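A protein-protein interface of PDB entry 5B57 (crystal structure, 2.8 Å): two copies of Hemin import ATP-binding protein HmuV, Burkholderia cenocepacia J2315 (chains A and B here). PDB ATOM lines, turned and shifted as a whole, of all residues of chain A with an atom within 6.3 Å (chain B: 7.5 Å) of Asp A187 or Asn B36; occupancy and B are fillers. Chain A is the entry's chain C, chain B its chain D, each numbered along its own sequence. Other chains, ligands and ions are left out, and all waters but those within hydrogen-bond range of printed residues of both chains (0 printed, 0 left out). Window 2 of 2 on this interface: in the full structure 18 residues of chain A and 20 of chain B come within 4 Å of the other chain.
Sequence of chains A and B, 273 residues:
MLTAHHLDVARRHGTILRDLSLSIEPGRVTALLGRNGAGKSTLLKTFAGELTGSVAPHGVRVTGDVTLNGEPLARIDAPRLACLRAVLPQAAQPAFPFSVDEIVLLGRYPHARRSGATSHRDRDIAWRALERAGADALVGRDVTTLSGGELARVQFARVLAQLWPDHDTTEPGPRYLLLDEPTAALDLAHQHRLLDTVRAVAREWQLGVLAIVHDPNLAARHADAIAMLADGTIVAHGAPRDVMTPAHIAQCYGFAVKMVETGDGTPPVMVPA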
ATOM      1  N   GLY A 149     -10.713  16.008  -0.683  1.00  0.00           N
ATOM      2  CA  GLY A 149     -11.968  15.980  -1.409  1.00  0.00           C
ATOM      3  C   GLY A 149     -11.771  15.878  -2.911  1.00  0.00           C
ATOM      4  O   GLY A 149     -12.435  15.092  -3.585  1.00  0.00           O
ATOM      5  N   THR A 183     -17.265   7.528   1.547  1.00  0.00           N
ATOM      6  CA  THR A 183     -18.062   8.707   1.773  1.00  0.00           C
ATOM      7  C   THR A 183     -17.570   9.540   2.954  1.00  0.00           C
ATOM      8  O   THR A 183     -17.834  10.745   2.990  1.00  0.00           O
ATOM      9  CB  THR A 183     -19.521   8.256   1.936  1.00  0.00           C
ATOM     10  OG1 THR A 183     -20.400   9.393   1.949  1.00  0.00           O
ATOM     11  CG2 THR A 183     -19.685   7.292   3.171  1.00  0.00           C
ATOM     12  N   ALA A 185     -14.944  11.600   5.472  1.00  0.00           N
ATOM     13  CA  ALA A 185     -13.952  12.635   5.202  1.00  0.00           C
ATOM     14  C   ALA A 185     -14.225  13.363   3.893  1.00  0.00           C
ATOM     15  O   ALA A 185     -13.337  14.017   3.334  1.00  0.00           O
ATOM     16  CB  ALA A 185     -12.520  12.073   5.211  1.00  0.00           C
ATOM     17  N   LEU A 186     -15.436  13.230   3.376  1.00  0.00           N
ATOM     18  CA  LEU A 186     -15.988  14.164   2.408  1.00  0.00           C
ATOM     19  C   LEU A 186     -16.928  15.084   3.173  1.00  0.00           C
ATOM     20  O   LEU A 186     -17.542  14.657   4.153  1.00  0.00           O
ATOM     21  CB  LEU A 186     -16.737  13.421   1.295  1.00  0.00           C
ATOM     22  CG  LEU A 186     -15.957  12.780   0.123  1.00  0.00           C
ATOM     23  CD1 LEU A 186     -14.717  12.054   0.570  1.00  0.00           C
ATOM     24  CD2 LEU A 186     -16.825  11.833  -0.679  1.00  0.00           C
ATOM     25  N   ASP A 187     -17.014  16.352   2.770  1.00  0.00           N
ATOM     26  CA  ASP A 187     -17.959  17.219   3.476  1.00  0.00           C
ATOM     27  C   ASP A 187     -19.393  16.859   3.065  1.00  0.00           C
ATOM     28  O   ASP A 187     -19.622  16.073   2.136  1.00  0.00           O
ATOM     29  CB  ASP A 187     -17.664  18.704   3.236  1.00  0.00           C
ATOM     30  CG  ASP A 187     -16.294  18.953   2.641  1.00  0.00           C
ATOM     31  OD1 ASP A 187     -15.855  18.118   1.818  1.00  0.00           O
ATOM     32  OD2 ASP A 187     -15.663  19.992   2.966  1.00  0.00           O
ATOM     33  N   LEU A 188     -20.363  17.429   3.798  1.00  0.00           N
ATOM     34  CA  LEU A 188     -21.751  16.980   3.700  1.00  0.00           C
ATOM     35  C   LEU A 188     -22.232  16.961   2.255  1.00  0.00           C
ATOM     36  O   LEU A 188     -22.594  15.910   1.723  1.00  0.00           O
ATOM     37  CB  LEU A 188     -22.655  17.881   4.536  1.00  0.00           C
ATOM     38  CG  LEU A 188     -22.536  17.831   6.040  1.00  0.00           C
ATOM     39  CD1 LEU A 188     -23.415  18.917   6.631  1.00  0.00           C
ATOM     40  CD2 LEU A 188     -22.962  16.467   6.539  1.00  0.00           C
ATOM     41  N   ALA A 189     -22.250  18.134   1.615  1.00  0.00           N
ATOM     42  CA  ALA A 189     -22.745  18.227   0.243  1.00  0.00           C
ATOM     43  C   ALA A 189     -22.070  17.201  -0.651  1.00  0.00           C
ATOM     44  O   ALA A 189     -22.725  16.550  -1.469  1.00  0.00           O
ATOM     45  CB  ALA A 189     -22.519  19.643  -0.283  1.00  0.00           C
ATOM     46  N   HIS A 190     -20.757  17.037  -0.480  1.00  0.00           N
ATOM     47  CA  HIS A 190     -19.985  16.055  -1.228  1.00  0.00           C
ATOM     48  C   HIS A 190     -20.524  14.632  -1.015  1.00  0.00           C
ATOM     49  O   HIS A 190     -20.712  13.883  -1.983  1.00  0.00           O
ATOM     50  CB  HIS A 190     -18.519  16.201  -0.801  1.00  0.00           C
ATOM     51  CG  HIS A 190     -17.520  15.456  -1.645  1.00  0.00           C
ATOM     52  ND1 HIS A 190     -17.866  14.503  -2.583  1.00  0.00           N
ATOM     53  CD2 HIS A 190     -16.165  15.522  -1.666  1.00  0.00           C
ATOM     54  CE1 HIS A 190     -16.770  14.020  -3.146  1.00  0.00           C
ATOM     55  NE2 HIS A 190     -15.724  14.618  -2.605  1.00  0.00           N
ATOM     56  N   GLN A 191     -20.804  14.236   0.243  1.00  0.00           N
ATOM     57  CA  GLN A 191     -21.222  12.848   0.465  1.00  0.00           C
ATOM     58  C   GLN A 191     -22.521  12.549  -0.269  1.00  0.00           C
ATOM     59  O   GLN A 191     -22.668  11.482  -0.872  1.00  0.00           O
ATOM     60  CB  GLN A 191     -21.409  12.498   1.948  1.00  0.00           C
ATOM     61  CG  GLN A 191     -20.634  13.257   2.979  1.00  0.00           C
ATOM     62  CD  GLN A 191     -20.809  12.650   4.379  1.00  0.00           C
ATOM     63  OE1 GLN A 191     -21.890  12.696   4.972  1.00  0.00           O
ATOM     64  NE2 GLN A 191     -19.744  12.071   4.902  1.00  0.00           N
ATOM     65  N   HIS A 192     -23.484  13.465  -0.216  1.00  0.00           N
ATOM     66  CA  HIS A 192     -24.739  13.199  -0.906  1.00  0.00           C
ATOM     67  C   HIS A 192     -24.522  13.173  -2.413  1.00  0.00           C
ATOM     68  O   HIS A 192     -25.075  12.299  -3.093  1.00  0.00           O
ATOM     69  CB  HIS A 192     -25.822  14.209  -0.474  1.00  0.00           C
ATOM     70  CG  HIS A 192     -26.278  14.021   0.948  1.00  0.00           C
ATOM     71  ND1 HIS A 192     -27.129  13.005   1.329  1.00  0.00           N
ATOM     72  CD2 HIS A 192     -25.947  14.674   2.089  1.00  0.00           C
ATOM     73  CE1 HIS A 192     -27.316  13.053   2.637  1.00  0.00           C
ATOM     74  NE2 HIS A 192     -26.610  14.057   3.124  1.00  0.00           N
ATOM     75  N   ARG A 193     -23.656  14.065  -2.938  1.00  0.00           N
ATOM     76  CA  ARG A 193     -23.348  14.092  -4.374  1.00  0.00           C
ATOM     77  C   ARG A 193     -22.892  12.728  -4.868  1.00  0.00           C
ATOM     78  O   ARG A 193     -23.390  12.232  -5.894  1.00  0.00           O
ATOM     79  CB  ARG A 193     -22.264  15.125  -4.685  1.00  0.00           C
ATOM     80  CG  ARG A 193     -22.725  16.552  -5.051  1.00  0.00           C
ATOM     81  CD  ARG A 193     -21.579  17.403  -5.687  1.00  0.00           C
ATOM     82  NE  ARG A 193     -20.500  17.838  -4.769  1.00  0.00           N
ATOM     83  CZ  ARG A 193     -19.262  17.312  -4.701  1.00  0.00           C
ATOM     84  NH1 ARG A 193     -18.901  16.291  -5.480  1.00  0.00           N
ATOM     85  NH2 ARG A 193     -18.369  17.808  -3.840  1.00  0.00           N
ATOM     86  N   GLY B  34     -17.474  23.412  10.396  1.00  0.00           N
ATOM     87  CA  GLY B  34     -16.986  23.994   9.158  1.00  0.00           C
ATOM     88  C   GLY B  34     -16.620  22.876   8.218  1.00  0.00           C
ATOM     89  O   GLY B  34     -16.519  21.713   8.618  1.00  0.00           O
ATOM     90  N   ARG B  35     -16.433  23.234   6.950  1.00  0.00           N
ATOM     91  CA  ARG B  35     -16.051  22.178   6.024  1.00  0.00           C
ATOM     92  C   ARG B  35     -14.532  22.061   5.964  1.00  0.00           C
ATOM     93  O   ARG B  35     -13.798  22.840   6.574  1.00  0.00           O
ATOM     94  CB  ARG B  35     -16.681  22.392   4.642  1.00  0.00           C
ATOM     95  CG  ARG B  35     -16.645  23.770   4.030  1.00  0.00           C
ATOM     96  CD  ARG B  35     -17.079  23.658   2.565  1.00  0.00           C
ATOM     97  NE  ARG B  35     -17.422  24.947   1.984  1.00  0.00           N
ATOM     98  CZ  ARG B  35     -16.558  25.769   1.388  1.00  0.00           C
ATOM     99  NH1 ARG B  35     -15.272  25.439   1.282  1.00  0.00           N
ATOM    100  NH2 ARG B  35     -16.985  26.932   0.895  1.00  0.00           N
ATOM    101  N   ASN B  36     -14.063  21.036   5.256  1.00  0.00           N
ATOM    102  CA  ASN B  36     -12.634  20.735   5.224  1.00  0.00           C
ATOM    103  C   ASN B  36     -11.858  21.883   4.604  1.00  0.00           C
ATOM    104  O   ASN B  36     -12.189  22.357   3.512  1.00  0.00           O
ATOM    105  CB  ASN B  36     -12.382  19.440   4.459  1.00  0.00           C
ATOM    106  CG  ASN B  36     -13.022  18.259   5.137  1.00  0.00           C
ATOM    107  OD1 ASN B  36     -13.219  18.286   6.357  1.00  0.00           O
ATOM    108  ND2 ASN B  36     -13.375  17.231   4.371  1.00  0.00           N
ATOM    109  N   GLY B  37     -10.840  22.346   5.321  1.00  0.00           N
ATOM    110  CA  GLY B  37     -10.090  23.498   4.879  1.00  0.00           C
ATOM    111  C   GLY B  37     -10.661  24.814   5.322  1.00  0.00           C
ATOM    112  O   GLY B  37     -10.295  25.855   4.766  1.00  0.00           O
ATOM    113  N   ALA B  38     -11.548  24.810   6.306  1.00  0.00           N
ATOM    114  CA  ALA B  38     -12.105  26.059   6.785  1.00  0.00           C
ATOM    115  C   ALA B  38     -11.252  26.698   7.871  1.00  0.00           C
ATOM    116  O   ALA B  38     -11.494  27.858   8.238  1.00  0.00           O
ATOM    117  CB  ALA B  38     -13.534  25.843   7.297  1.00  0.00           C
ATOM    118  N   GLY B  39     -10.278  25.970   8.390  1.00  0.00           N
ATOM    119  CA  GLY B  39      -9.448  26.463   9.455  1.00  0.00           C
ATOM    120  C   GLY B  39      -9.870  26.071  10.848  1.00  0.00           C
ATOM    121  O   GLY B  39      -9.405  26.705  11.803  1.00  0.00           O
ATOM    122  N   LYS B  40     -10.750  25.067  10.990  1.00  0.00           N
ATOM    123  CA  LYS B  40     -11.080  24.493  12.298  1.00  0.00           C
ATOM    124  C   LYS B  40      -9.826  24.091  13.076  1.00  0.00           C
ATOM    125  O   LYS B  40      -9.614  24.514  14.217  1.00  0.00           O
ATOM    126  CB  LYS B  40     -11.974  23.263  12.127  1.00  0.00           C
ATOM    127  CG  LYS B  40     -13.451  23.475  11.856  1.00  0.00           C
ATOM    128  CD  LYS B  40     -14.085  22.117  11.594  1.00  0.00           C
ATOM    129  CE  LYS B  40     -13.663  21.620  10.221  1.00  0.00           C
ATOM    130  NZ  LYS B  40     -13.822  20.150   9.985  1.00  0.00           N
ATOM    131  N   GLU B 181     -11.507  16.621  17.150  1.00  0.00           N
ATOM    132  CA  GLU B 181     -12.245  15.548  16.495  1.00  0.00           C
ATOM    133  C   GLU B 181     -12.057  14.180  17.147  1.00  0.00           C
ATOM    134  O   GLU B 181     -11.517  13.255  16.526  1.00  0.00           O
ATOM    135  CB  GLU B 181     -11.866  15.499  15.025  1.00  0.00           C
ATOM    136  CG  GLU B 181     -13.072  15.226  14.161  1.00  0.00           C
ATOM    137  CD  GLU B 181     -12.847  15.556  12.707  1.00  0.00           C
ATOM    138  OE1 GLU B 181     -11.734  15.266  12.184  1.00  0.00           O
ATOM    139  OE2 GLU B 181     -13.796  16.107  12.095  1.00  0.00           O
ATOM    140  N   LEU B 229     -17.735  27.902  11.007  1.00  0.00           N
ATOM    141  CA  LEU B 229     -16.540  28.426  10.335  1.00  0.00           C
ATOM    142  C   LEU B 229     -16.696  28.330   8.818  1.00  0.00           C
ATOM    143  O   LEU B 229     -16.841  27.227   8.271  1.00  0.00           O
ATOM    144  CB  LEU B 229     -15.296  27.653  10.761  1.00  0.00           C
ATOM    145  CG  LEU B 229     -14.012  28.463  10.852  1.00  0.00           C
ATOM    146  CD1 LEU B 229     -14.196  29.523  11.907  1.00  0.00           C
ATOM    147  CD2 LEU B 229     -12.852  27.570  11.225  1.00  0.00           C
ATOM    148  N   CYS B 252     -22.352  27.900   5.478  1.00  0.00           N
ATOM    149  CA  CYS B 252     -21.255  27.200   6.107  1.00  0.00           C
ATOM    150  C   CYS B 252     -20.819  26.003   5.271  1.00  0.00           C
ATOM    151  O   CYS B 252     -19.630  25.842   4.983  1.00  0.00           O
ATOM    152  CB  CYS B 252     -21.669  26.757   7.509  1.00  0.00           C
ATOM    153  SG  CYS B 252     -20.435  25.774   8.342  1.00  0.00           S
ATOM    154  N   TYR B 253     -21.768  25.168   4.862  1.00  0.00           N
ATOM    155  CA  TYR B 253     -21.477  23.936   4.136  1.00  0.00           C
ATOM    156  C   TYR B 253     -21.825  23.973   2.653  1.00  0.00           C
ATOM    157  O   TYR B 253     -21.589  22.973   1.967  1.00  0.00           O
ATOM    158  CB  TYR B 253     -22.225  22.758   4.764  1.00  0.00           C
ATOM    159  CG  TYR B 253     -21.787  22.410   6.151  1.00  0.00           C
ATOM    160  CD1 TYR B 253     -20.503  21.997   6.400  1.00  0.00           C
ATOM    161  CD2 TYR B 253     -22.677  22.461   7.210  1.00  0.00           C
ATOM    162  CE1 TYR B 253     -20.104  21.664   7.668  1.00  0.00           C
ATOM    163  CE2 TYR B 253     -22.288  22.127   8.480  1.00  0.00           C
ATOM    164  CZ  TYR B 253     -20.996  21.727   8.699  1.00  0.00           C
ATOM    165  OH  TYR B 253     -20.588  21.387   9.963  1.00  0.00           O
ATOM    166  N   PHE B 255     -24.714  23.669   1.424  1.00  0.00           N
ATOM    167  CA  PHE B 255     -25.504  22.453   1.496  1.00  0.00           C
ATOM    168  C   PHE B 255     -26.924  22.838   1.894  1.00  0.00           C
ATOM    169  O   PHE B 255     -27.140  23.507   2.912  1.00  0.00           O
ATOM    170  CB  PHE B 255     -24.871  21.497   2.502  1.00  0.00           C
ATOM    171  CG  PHE B 255     -25.567  20.195   2.627  1.00  0.00           C
ATOM    172  CD1 PHE B 255     -26.298  19.671   1.565  1.00  0.00           C
ATOM    173  CD2 PHE B 255     -25.489  19.488   3.814  1.00  0.00           C
ATOM    174  CE1 PHE B 255     -26.946  18.456   1.686  1.00  0.00           C
ATOM    175  CE2 PHE B 255     -26.124  18.284   3.952  1.00  0.00           C
ATOM    176  CZ  PHE B 255     -26.866  17.761   2.879  1.00  0.00           C
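O of Ala A185 lies within hydrogen-bond range of ND2 of Asn B36 (3.4 Å). The backbone NH (N) of Asn B36 lies within hydrogen-bond range of the side-chain carboxylate (OD2) of Asp A187 (3.0 Å).
Among the printed residues, pairs that only touch across the chains: Asp A187 with Arg B35, Leu A188 with Tyr B253, Leu A188 with Phe B255 and His A192 with Phe B255.
Printed residues of chain B within 4 Å of Leu A188: Tyr B253 and Phe B255. Of the printed residues of chain A, Arg B35 touches Asp A187. Asn B36 touches just these residues of chain A: Ala A185 (3.4 Å) and Asp A187 (3.0 Å). Ala B38 touches none of the printed residues of chain A. Glu B181 touches none of the printed residues of chain A. Printed residues of chain A within 4 Å of Tyr B253: Leu A188. The nearest residue of chain B that does not touch Asp A187 is Tyr B253 (5.4 Å). The nearest printed residue of chain B that does not touch Ala A185 is Glu B181 (7.7 Å).
Of the 12 printed residues of chain B, 4 touch a printed residue of chain A. Hydrophobic or aromatic side chains of chain B within 4 Å of the printed part of chain A: Tyr B253 and Phe B255. Of the 11 printed residues of chain A, 4 touch a printed residue of chain B. Hydrophobic or aromatic side chains of chain A within 4 Å of the printed part of chain B: Leu A188 and His A192. Among the printed residues, no Asp or Glu carboxylate lies within 4 Å of a Lys or Arg side-chain nitrogen of the other chain.
No position is printed for both chains.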
